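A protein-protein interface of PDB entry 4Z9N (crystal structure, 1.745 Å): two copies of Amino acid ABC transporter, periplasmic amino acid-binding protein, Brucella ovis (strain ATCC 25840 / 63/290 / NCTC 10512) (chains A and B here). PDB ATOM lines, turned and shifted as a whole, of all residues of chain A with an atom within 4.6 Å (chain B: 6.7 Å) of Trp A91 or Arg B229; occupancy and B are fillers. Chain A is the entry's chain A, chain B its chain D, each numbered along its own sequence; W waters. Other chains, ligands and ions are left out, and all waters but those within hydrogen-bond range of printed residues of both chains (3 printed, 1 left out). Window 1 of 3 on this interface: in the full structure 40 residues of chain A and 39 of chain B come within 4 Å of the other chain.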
ATOM      1  N   THR A  89      17.378 -19.811  11.902  1.00  0.00           N
ATOM      2  CA  THR A  89      17.612 -18.574  12.635  1.00  0.00           C
ATOM      3  C   THR A  89      17.502 -17.361  11.730  1.00  0.00           C
ATOM      4  O   THR A  89      18.251 -17.233  10.770  1.00  0.00           O
ATOM      5  CB  THR A  89      18.997 -18.594  13.329  1.00  0.00           C
ATOM      6  OG1 THR A  89      18.962 -19.566  14.383  1.00  0.00           O
ATOM      7  CG2 THR A  89      19.355 -17.209  13.901  1.00  0.00           C
ATOM      8  N   THR A  90      16.574 -16.465  12.064  1.00  0.00           N
ATOM      9  CA  THR A  90      16.248 -15.343  11.191  1.00  0.00           C
ATOM     10  C   THR A  90      17.321 -14.267  11.227  1.00  0.00           C
ATOM     11  O   THR A  90      17.771 -13.876  12.290  1.00  0.00           O
ATOM     12  CB  THR A  90      14.906 -14.720  11.583  1.00  0.00           C
ATOM     13  OG1 THR A  90      13.893 -15.721  11.478  1.00  0.00           O
ATOM     14  CG2 THR A  90      14.559 -13.544  10.654  1.00  0.00           C
ATOM     15  N   TRP A  91      17.728 -13.825  10.045  1.00  0.00           N
ATOM     16  CA  TRP A  91      18.602 -12.669   9.879  1.00  0.00           C
ATOM     17  C   TRP A  91      17.784 -11.401  10.136  1.00  0.00           C
ATOM     18  O   TRP A  91      16.804 -11.162   9.418  1.00  0.00           O
ATOM     19  CB  TRP A  91      19.160 -12.681   8.458  1.00  0.00           C
ATOM     20  CG  TRP A  91      20.210 -11.676   8.108  1.00  0.00           C
ATOM     21  CD1 TRP A  91      20.580 -10.544   8.793  1.00  0.00           C
ATOM     22  CD2 TRP A  91      21.018 -11.722   6.938  1.00  0.00           C
ATOM     23  NE1 TRP A  91      21.591  -9.891   8.108  1.00  0.00           N
ATOM     24  CE2 TRP A  91      21.881 -10.607   6.973  1.00  0.00           C
ATOM     25  CE3 TRP A  91      21.115 -12.624   5.871  1.00  0.00           C
ATOM     26  CZ2 TRP A  91      22.813 -10.358   5.969  1.00  0.00           C
ATOM     27  CZ3 TRP A  91      22.038 -12.375   4.874  1.00  0.00           C
ATOM     28  CH2 TRP A  91      22.880 -11.258   4.934  1.00  0.00           C
ATOM     29  N   THR A  92      18.175 -10.613  11.146  1.00  0.00           N
ATOM     30  CA  THR A  92      17.525  -9.326  11.445  1.00  0.00           C
ATOM     31  C   THR A  92      18.603  -8.275  11.665  1.00  0.00           C
ATOM     32  O   THR A  92      19.777  -8.617  11.891  1.00  0.00           O
ATOM     33  CB  THR A  92      16.633  -9.377  12.714  1.00  0.00           C
ATOM     34  OG1 THR A  92      17.477  -9.474  13.867  1.00  0.00           O
ATOM     35  CG2 THR A  92      15.689 -10.571  12.672  1.00  0.00           C
ATOM     36  N   ASP A  96      22.426  -8.662  13.415  1.00  0.00           N
ATOM     37  CA  ASP A  96      23.541  -8.360  12.513  1.00  0.00           C
ATOM     38  C   ASP A  96      24.467  -7.303  13.141  1.00  0.00           C
ATOM     39  O   ASP A  96      25.678  -7.305  12.912  1.00  0.00           O
ATOM     40  CB  ASP A  96      22.969  -7.880  11.171  1.00  0.00           C
ATOM     41  CG  ASP A  96      23.925  -8.059   9.995  1.00  0.00           C
ATOM     42  OD1 ASP A  96      25.073  -8.531  10.155  1.00  0.00           O
ATOM     43  OD2 ASP A  96      23.499  -7.716   8.875  1.00  0.00           O
ATOM     44  N   ASP A 102      27.672 -12.200  11.824  1.00  0.00           N
ATOM     45  CA  ASP A 102      27.374 -11.901  10.423  1.00  0.00           C
ATOM     46  C   ASP A 102      26.595 -13.059   9.833  1.00  0.00           C
ATOM     47  O   ASP A 102      26.533 -14.157  10.413  1.00  0.00           O
ATOM     48  CB  ASP A 102      28.638 -11.705   9.577  1.00  0.00           C
ATOM     49  CG  ASP A 102      29.198 -10.296   9.622  1.00  0.00           C
ATOM     50  OD1 ASP A 102      28.457  -9.318   9.837  1.00  0.00           O
ATOM     51  OD2 ASP A 102      30.417 -10.180   9.389  1.00  0.00           O
ATOM     52  N   PHE A 103      26.036 -12.833   8.652  1.00  0.00           N
ATOM     53  CA  PHE A 103      25.269 -13.862   7.986  1.00  0.00           C
ATOM     54  C   PHE A 103      25.822 -14.085   6.600  1.00  0.00           C
ATOM     55  O   PHE A 103      25.986 -13.133   5.827  1.00  0.00           O
ATOM     56  CB  PHE A 103      23.778 -13.472   7.936  1.00  0.00           C
ATOM     57  CG  PHE A 103      23.149 -13.352   9.297  1.00  0.00           C
ATOM     58  CD1 PHE A 103      23.259 -12.174  10.027  1.00  0.00           C
ATOM     59  CD2 PHE A 103      22.466 -14.427   9.858  1.00  0.00           C
ATOM     60  CE1 PHE A 103      22.706 -12.071  11.288  1.00  0.00           C
ATOM     61  CE2 PHE A 103      21.890 -14.325  11.120  1.00  0.00           C
ATOM     62  CZ  PHE A 103      22.008 -13.143  11.831  1.00  0.00           C
ATOM     63  N   GLY A 105      24.522 -16.004   4.155  1.00  0.00           N
ATOM     64  CA  GLY A 105      23.561 -16.333   3.119  1.00  0.00           C
ATOM     65  C   GLY A 105      22.232 -16.703   3.739  1.00  0.00           C
ATOM     66  O   GLY A 105      22.137 -16.859   4.964  1.00  0.00           O
ATOM     67  N   ILE A 106      21.216 -16.836   2.896  1.00  0.00           N
ATOM     68  CA  ILE A 106      19.873 -17.194   3.362  1.00  0.00           C
ATOM     69  C   ILE A 106      19.532 -18.555   2.740  1.00  0.00           C
ATOM     70  O   ILE A 106      19.347 -18.643   1.517  1.00  0.00           O
ATOM     71  CB  ILE A 106      18.827 -16.102   2.977  1.00  0.00           C
ATOM     72  CG1 ILE A 106      19.111 -14.781   3.718  1.00  0.00           C
ATOM     73  CG2 ILE A 106      17.381 -16.586   3.264  1.00  0.00           C
ATOM     74  CD1 ILE A 106      18.386 -13.564   3.106  1.00  0.00           C
ATOM     75  N   PRO A 212      13.900 -14.659   7.018  1.00  0.00           N
ATOM     76  CA  PRO A 212      14.944 -15.293   6.198  1.00  0.00           C
ATOM     77  C   PRO A 212      15.908 -16.052   7.100  1.00  0.00           C
ATOM     78  O   PRO A 212      16.584 -15.425   7.929  1.00  0.00           O
ATOM     79  CB  PRO A 212      15.613 -14.101   5.504  1.00  0.00           C
ATOM     80  CG  PRO A 212      15.386 -12.929   6.470  1.00  0.00           C
ATOM     81  CD  PRO A 212      14.025 -13.190   7.060  1.00  0.00           C
ATOM     82  N   GLY A 214      19.167 -17.580   8.228  1.00  0.00           N
ATOM     83  CA  GLY A 214      20.520 -17.195   7.876  1.00  0.00           C
ATOM     84  C   GLY A 214      21.594 -18.178   8.288  1.00  0.00           C
ATOM     85  O   GLY A 214      21.515 -18.806   9.344  1.00  0.00           O
ATOM     86  N   ASP B 102      34.472  -7.271   0.571  1.00  0.00           N
ATOM     87  CA  ASP B 102      33.182  -7.905   0.849  1.00  0.00           C
ATOM     88  C   ASP B 102      32.084  -7.137   0.108  1.00  0.00           C
ATOM     89  O   ASP B 102      32.299  -6.032  -0.404  1.00  0.00           O
ATOM     90  CB  ASP B 102      32.864  -7.907   2.353  1.00  0.00           C
ATOM     91  CG  ASP B 102      33.507  -9.060   3.108  1.00  0.00           C
ATOM     92  OD1 ASP B 102      33.738 -10.138   2.527  1.00  0.00           O
ATOM     93  OD2 ASP B 102      33.779  -8.875   4.310  1.00  0.00           O
ATOM     94  N   PHE B 103      30.893  -7.708   0.094  1.00  0.00           N
ATOM     95  CA  PHE B 103      29.755  -7.087  -0.579  1.00  0.00           C
ATOM     96  C   PHE B 103      28.616  -6.982   0.413  1.00  0.00           C
ATOM     97  O   PHE B 103      28.286  -7.961   1.083  1.00  0.00           O
ATOM     98  CB  PHE B 103      29.351  -7.899  -1.812  1.00  0.00           C
ATOM     99  CG  PHE B 103      30.415  -7.937  -2.867  1.00  0.00           C
ATOM    100  CD1 PHE B 103      31.445  -8.877  -2.811  1.00  0.00           C
ATOM    101  CD2 PHE B 103      30.409  -7.016  -3.902  1.00  0.00           C
ATOM    102  CE1 PHE B 103      32.443  -8.885  -3.780  1.00  0.00           C
ATOM    103  CE2 PHE B 103      31.402  -7.032  -4.867  1.00  0.00           C
ATOM    104  CZ  PHE B 103      32.410  -7.949  -4.805  1.00  0.00           C
ATOM    105  N   ALA B 104      28.029  -5.797   0.515  1.00  0.00           N
ATOM    106  CA  ALA B 104      27.046  -5.533   1.554  1.00  0.00           C
ATOM    107  C   ALA B 104      25.620  -5.790   1.063  1.00  0.00           C
ATOM    108  O   ALA B 104      24.673  -5.773   1.847  1.00  0.00           O
ATOM    109  CB  ALA B 104      27.190  -4.117   2.053  1.00  0.00           C
ATOM    110  N   GLY B 105      25.466  -6.063  -0.228  1.00  0.00           N
ATOM    111  CA  GLY B 105      24.133  -6.198  -0.798  1.00  0.00           C
ATOM    112  C   GLY B 105      24.201  -6.081  -2.312  1.00  0.00           C
ATOM    113  O   GLY B 105      25.245  -5.737  -2.856  1.00  0.00           O
ATOM    114  N   LEU B 215      27.246  -3.743  -3.577  1.00  0.00           N
ATOM    115  CA  LEU B 215      27.733  -2.650  -2.753  1.00  0.00           C
ATOM    116  C   LEU B 215      29.036  -3.094  -2.120  1.00  0.00           C
ATOM    117  O   LEU B 215      29.041  -3.940  -1.225  1.00  0.00           O
ATOM    118  CB  LEU B 215      26.690  -2.292  -1.694  1.00  0.00           C
ATOM    119  CG  LEU B 215      25.320  -2.004  -2.318  1.00  0.00           C
ATOM    120  CD1 LEU B 215      24.288  -1.791  -1.241  1.00  0.00           C
ATOM    121  CD2 LEU B 215      25.380  -0.801  -3.256  1.00  0.00           C
ATOM    122  N   ALA B 222      33.267  -4.814  10.042  1.00  0.00           N
ATOM    123  CA  ALA B 222      31.878  -5.269  10.059  1.00  0.00           C
ATOM    124  C   ALA B 222      30.912  -4.119  10.296  1.00  0.00           C
ATOM    125  O   ALA B 222      29.822  -4.090   9.716  1.00  0.00           O
ATOM    126  CB  ALA B 222      31.682  -6.349  11.126  1.00  0.00           C
ATOM    127  N   TRP B 224      31.180  -1.010   9.384  1.00  0.00           N
ATOM    128  CA  TRP B 224      31.004  -0.263   8.142  1.00  0.00           C
ATOM    129  C   TRP B 224      30.159  -1.040   7.128  1.00  0.00           C
ATOM    130  O   TRP B 224      29.292  -0.458   6.462  1.00  0.00           O
ATOM    131  CB  TRP B 224      32.361   0.109   7.524  1.00  0.00           C
ATOM    132  CG  TRP B 224      32.196   0.920   6.286  1.00  0.00           C
ATOM    133  CD1 TRP B 224      32.598   0.586   5.030  1.00  0.00           C
ATOM    134  CD2 TRP B 224      31.538   2.191   6.175  1.00  0.00           C
ATOM    135  NE1 TRP B 224      32.252   1.576   4.139  1.00  0.00           N
ATOM    136  CE2 TRP B 224      31.602   2.574   4.821  1.00  0.00           C
ATOM    137  CE3 TRP B 224      30.927   3.053   7.097  1.00  0.00           C
ATOM    138  CZ2 TRP B 224      31.064   3.777   4.357  1.00  0.00           C
ATOM    139  CZ3 TRP B 224      30.390   4.250   6.635  1.00  0.00           C
ATOM    140  CH2 TRP B 224      30.467   4.602   5.280  1.00  0.00           C
ATOM    141  N   ALA B 225      30.406  -2.341   6.995  1.00  0.00           N
ATOM    142  CA  ALA B 225      29.589  -3.175   6.108  1.00  0.00           C
ATOM    143  C   ALA B 225      28.126  -3.165   6.544  1.00  0.00           C
ATOM    144  O   ALA B 225      27.219  -3.128   5.696  1.00  0.00           O
ATOM    145  CB  ALA B 225      30.113  -4.605   6.065  1.00  0.00           C
ATOM    146  N   ASP B 226      27.895  -3.207   7.859  1.00  0.00           N
ATOM    147  CA  ASP B 226      26.522  -3.141   8.385  1.00  0.00           C
ATOM    148  C   ASP B 226      25.813  -1.850   7.964  1.00  0.00           C
ATOM    149  O   ASP B 226      24.632  -1.871   7.611  1.00  0.00           O
ATOM    150  CB  ASP B 226      26.512  -3.269   9.915  1.00  0.00           C
ATOM    151  CG  ASP B 226      26.856  -4.685  10.409  1.00  0.00           C
ATOM    152  OD1 ASP B 226      27.024  -5.604   9.588  1.00  0.00           O
ATOM    153  OD2 ASP B 226      26.984  -4.867  11.635  1.00  0.00           O
ATOM    154  N   VAL B 227      26.527  -0.727   8.004  1.00  0.00           N
ATOM    155  CA  VAL B 227      25.927   0.566   7.633  1.00  0.00           C
ATOM    156  C   VAL B 227      25.502   0.557   6.167  1.00  0.00           C
ATOM    157  O   VAL B 227      24.411   1.015   5.807  1.00  0.00           O
ATOM    158  CB  VAL B 227      26.906   1.751   7.897  1.00  0.00           C
ATOM    159  CG1 VAL B 227      26.382   3.028   7.244  1.00  0.00           C
ATOM    160  CG2 VAL B 227      27.137   1.950   9.393  1.00  0.00           C
ATOM    161  N   VAL B 228      26.361   0.014   5.310  1.00  0.00           N
ATOM    162  CA  VAL B 228      26.067   0.010   3.879  1.00  0.00           C
ATOM    163  C   VAL B 228      24.952  -0.980   3.604  1.00  0.00           C
ATOM    164  O   VAL B 228      24.004  -0.670   2.887  1.00  0.00           O
ATOM    165  CB  VAL B 228      27.314  -0.313   3.053  1.00  0.00           C
ATOM    166  CG1 VAL B 228      26.958  -0.464   1.562  1.00  0.00           C
ATOM    167  CG2 VAL B 228      28.394   0.782   3.262  1.00  0.00           C
ATOM    168  N   ARG B 229      25.062  -2.162   4.198  1.00  0.00           N
ATOM    169  CA  ARG B 229      24.042  -3.202   4.048  1.00  0.00           C
ATOM    170  C   ARG B 229      22.659  -2.727   4.478  1.00  0.00           C
ATOM    171  O   ARG B 229      21.636  -2.976   3.821  1.00  0.00           O
ATOM    172  CB  ARG B 229      24.409  -4.431   4.877  1.00  0.00           C
ATOM    173  CG  ARG B 229      23.321  -5.512   4.841  1.00  0.00           C
ATOM    174  CD  ARG B 229      23.744  -6.787   5.573  1.00  0.00           C
ATOM    175  NE  ARG B 229      25.131  -7.122   5.295  1.00  0.00           N
ATOM    176  CZ  ARG B 229      26.126  -7.005   6.169  1.00  0.00           C
ATOM    177  NH1 ARG B 229      25.896  -6.615   7.415  1.00  0.00           N
ATOM    178  NH2 ARG B 229      27.357  -7.305   5.796  1.00  0.00           N
ATOM    179  N   TRP B 230      22.615  -2.052   5.610  1.00  0.00           N
ATOM    180  CA  TRP B 230      21.324  -1.738   6.162  1.00  0.00           C
ATOM    181  C   TRP B 230      20.751  -0.445   5.588  1.00  0.00           C
ATOM    182  O   TRP B 230      19.542  -0.259   5.631  1.00  0.00           O
ATOM    183  CB  TRP B 230      21.413  -1.747   7.685  1.00  0.00           C
ATOM    184  CG  TRP B 230      21.360  -3.163   8.088  1.00  0.00           C
ATOM    185  CD1 TRP B 230      22.406  -3.961   8.464  1.00  0.00           C
ATOM    186  CD2 TRP B 230      20.207  -4.013   8.034  1.00  0.00           C
ATOM    187  NE1 TRP B 230      21.966  -5.243   8.683  1.00  0.00           N
ATOM    188  CE2 TRP B 230      20.618  -5.302   8.436  1.00  0.00           C
ATOM    189  CE3 TRP B 230      18.858  -3.799   7.718  1.00  0.00           C
ATOM    190  CZ2 TRP B 230      19.732  -6.382   8.512  1.00  0.00           C
ATOM    191  CZ3 TRP B 230      17.975  -4.867   7.805  1.00  0.00           C
ATOM    192  CH2 TRP B 230      18.416  -6.147   8.198  1.00  0.00           C
ATOM    193  N   THR B 231      21.591   0.393   4.979  1.00  0.00           N
ATOM    194  CA  THR B 231      21.077   1.456   4.111  1.00  0.00           C
ATOM    195  C   THR B 231      20.274   0.828   2.959  1.00  0.00           C
ATOM    196  O   THR B 231      19.126   1.204   2.712  1.00  0.00           O
ATOM    197  CB  THR B 231      22.205   2.339   3.546  1.00  0.00           C
ATOM    198  OG1 THR B 231      22.830   3.044   4.619  1.00  0.00           O
ATOM    199  CG2 THR B 231      21.654   3.347   2.532  1.00  0.00           C
ATOM    200  N   HIS B 232      20.887  -0.133   2.266  1.00  0.00           N
ATOM    201  CA  HIS B 232      20.216  -0.873   1.196  1.00  0.00           C
ATOM    202  C   HIS B 232      18.902  -1.513   1.636  1.00  0.00           C
ATOM    203  O   HIS B 232      17.875  -1.383   0.968  1.00  0.00           O
ATOM    204  CB  HIS B 232      21.162  -1.952   0.665  1.00  0.00           C
ATOM    205  CG  HIS B 232      20.530  -2.914  -0.290  1.00  0.00           C
ATOM    206  ND1 HIS B 232      19.976  -2.527  -1.493  1.00  0.00           N
ATOM    207  CD2 HIS B 232      20.440  -4.269  -0.252  1.00  0.00           C
ATOM    208  CE1 HIS B 232      19.543  -3.600  -2.138  1.00  0.00           C
ATOM    209  NE2 HIS B 232      19.816  -4.668  -1.406  1.00  0.00           N
ATOM    210  N   ASN B 233      18.927  -2.205   2.762  1.00  0.00           N
ATOM    211  CA  ASN B 233      17.732  -2.932   3.162  1.00  0.00           C
ATOM    212  C   ASN B 233      16.669  -1.980   3.686  1.00  0.00           C
ATOM    213  O   ASN B 233      15.479  -2.251   3.538  1.00  0.00           O
ATOM    214  CB  ASN B 233      18.087  -4.018   4.176  1.00  0.00           C
ATOM    215  CG  ASN B 233      18.700  -5.235   3.501  1.00  0.00           C
ATOM    216  OD1 ASN B 233      17.980  -6.053   2.938  1.00  0.00           O
ATOM    217  ND2 ASN B 233      20.039  -5.340   3.521  1.00  0.00           N
ATOM    218  N   ALA B 234      17.091  -0.838   4.234  1.00  0.00           N
ATOM    219  CA  ALA B 234      16.135   0.187   4.618  1.00  0.00           C
ATOM    220  C   ALA B 234      15.411   0.696   3.377  1.00  0.00           C
ATOM    221  O   ALA B 234      14.190   0.886   3.400  1.00  0.00           O
ATOM    222  CB  ALA B 234      16.817   1.346   5.351  1.00  0.00           C
ATOM    223  N   ILE B 325      15.705  -7.387   4.106  1.00  0.00           N
ATOM    224  CA  ILE B 325      15.861  -8.186   5.310  1.00  0.00           C
ATOM    225  C   ILE B 325      15.206  -7.404   6.443  1.00  0.00           C
ATOM    226  O   ILE B 325      15.269  -6.181   6.453  1.00  0.00           O
ATOM    227  CB  ILE B 325      17.374  -8.500   5.539  1.00  0.00           C
ATOM    228  CG1 ILE B 325      17.941  -9.225   4.322  1.00  0.00           C
ATOM    229  CG2 ILE B 325      17.602  -9.354   6.772  1.00  0.00           C
ATOM    230  CD1 ILE B 325      19.437  -9.357   4.361  1.00  0.00           C
ATOM    231  N   PRO B 326      14.516  -8.094   7.366  1.00  0.00           N
ATOM    232  CA  PRO B 326      13.711  -7.347   8.338  1.00  0.00           C
ATOM    233  C   PRO B 326      14.488  -6.461   9.304  1.00  0.00           C
ATOM    234  O   PRO B 326      15.506  -6.858   9.861  1.00  0.00           O
ATOM    235  CB  PRO B 326      12.977  -8.449   9.108  1.00  0.00           C
ATOM    236  CG  PRO B 326      13.768  -9.715   8.849  1.00  0.00           C
ATOM    237  CD  PRO B 326      14.276  -9.546   7.446  1.00  0.00           C
ATOM    238  N   VAL B 327      13.967  -5.256   9.496  1.00  0.00           N
ATOM    239  CA  VAL B 327      14.491  -4.319  10.475  1.00  0.00           C
ATOM    240  C   VAL B 327      13.785  -4.649  11.780  1.00  0.00           C
ATOM    241  O   VAL B 327      12.738  -4.089  12.114  1.00  0.00           O
ATOM    242  CB  VAL B 327      14.276  -2.871  10.001  1.00  0.00           C
ATOM    243  CG1 VAL B 327      14.694  -1.873  11.059  1.00  0.00           C
ATOM    244  CG2 VAL B 327      15.090  -2.656   8.729  1.00  0.00           C
ATOM    245  N   ARG B 328      14.377  -5.591  12.505  1.00  0.00           N
ATOM    246  CA  ARG B 328      13.687  -6.313  13.567  1.00  0.00           C
ATOM    247  C   ARG B 328      14.664  -6.608  14.693  1.00  0.00           C
ATOM    248  O   ARG B 328      15.881  -6.510  14.489  1.00  0.00           O
ATOM    249  CB  ARG B 328      13.072  -7.608  13.000  1.00  0.00           C
ATOM    250  CG  ARG B 328      12.685  -8.710  14.011  1.00  0.00           C
ATOM    251  CD  ARG B 328      11.275  -8.545  14.586  1.00  0.00           C
ATOM    252  NE  ARG B 328      11.218  -7.531  15.635  1.00  0.00           N
ATOM    253  CZ  ARG B 328      10.100  -7.086  16.199  1.00  0.00           C
ATOM    254  NH1 ARG B 328      10.164  -6.151  17.153  1.00  0.00           N
ATOM    255  NH2 ARG B 328       8.919  -7.573  15.820  1.00  0.00           N
ATOM    256  OXT ARG B 328      14.263  -6.927  15.819  1.00  0.00           O
HETATM  257  O   HOH W   1      26.418 -10.238   5.313  1.00  0.00           O
HETATM  258  O   HOH W   2      15.835  -9.425  16.089  1.00  0.00           O
HETATM  259  O   HOH W   3      26.016 -10.000   7.943  1.00  0.00           O
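The side-chain hydroxyl (OG1) of Thr A92 sits at hydrogen-bond distance from the chain-end carboxylate (O) of Arg B328 (3.4 Å). O of Asp A96 lies close to OD2 of Asp B226 (3.0 Å). NH1 of Arg B229 is in salt-bridge range of OD2 of Asp A96. The side-chain carboxylate (OD2) of Asp A96 sits at hydrogen-bond distance from the indole nitrogen (NE1) of Trp B230 (2.9 Å).
The backbone carbonyl oxygen of Arg B229 is in hydrogen-bond range of the side-chain amide nitrogen of Asn B233 (2.9 Å). The side-chain carboxylate (OD2) of Asp A96 is in hydrogen-bond range of the indole nitrogen (NE1) of Trp A91 (3.0 Å). The side-chain amide oxygen (OD1) of Asn B233 lies within hydrogen-bond range of the backbone NH (N) of Ile B325, 2.9 Å away. The side-chain carboxylate (OD1) of Asp B226 lies within salt-bridge range of the guanidinium group (NH1) of Arg B229, at 2.6 Å. The backbone NH (N) of Trp A91 sits at hydrogen-bond distance from the backbone carbonyl oxygen (O) of Pro A212.
Among the printed residues, pairs that only touch across the chains: Trp A91 with Arg B229, Trp A91 with Trp B230, Trp A91 with Ile B325, Trp A91 with Pro B326, Thr A92 with Trp B230, Thr A92 with Pro B326, Asp A102 with Asp B226 and Pro A212 with Pro B326.
Printed residues of chain B within 4 Å of Trp A91: Arg B229 (3.7 Å), Trp B230 (3.99 Å), Ile B325 (3.3 Å) and Pro B326 (3.4 Å). Of the printed residues of chain A, Asp B226 touches Asp A96 and Asp A102. Arg B229 touches two residues of chain A. Of the printed residues of chain A, Trp B230 touches Trp A91, Thr A92 and Asp A96. The nearest printed residue of chain B that does not touch Trp A91 is Asn B233 (6.2 Å).
Of the 11 printed residues of chain A, 5 touch a printed residue of chain B. Hydrophobic or aromatic side chains of chain B that line the printed part of chain A: Trp B230, Ile B325 and Pro B326. Among the printed residues, 12 pairs touch across the chains.
Positions printed for both chains: 102, 103 and 105. Of the 12 pairs that touch across the chains among the printed residues, none has its exchanged pair printed and touching as well.
Water W2 bridges OG1 of Thr A92 (2.8 Å) and OXT of Arg B328 (3.0 Å). Water W3 lies within hydrogen-bond range of OD1 of Asp A96, N of Phe A103, OD1 of Asp A102 and NH1 of Arg B229. Water W1 lies within hydrogen-bond range of O of Phe A103 (3.0 Å) and NH2 of Arg B229 (3.1 Å).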
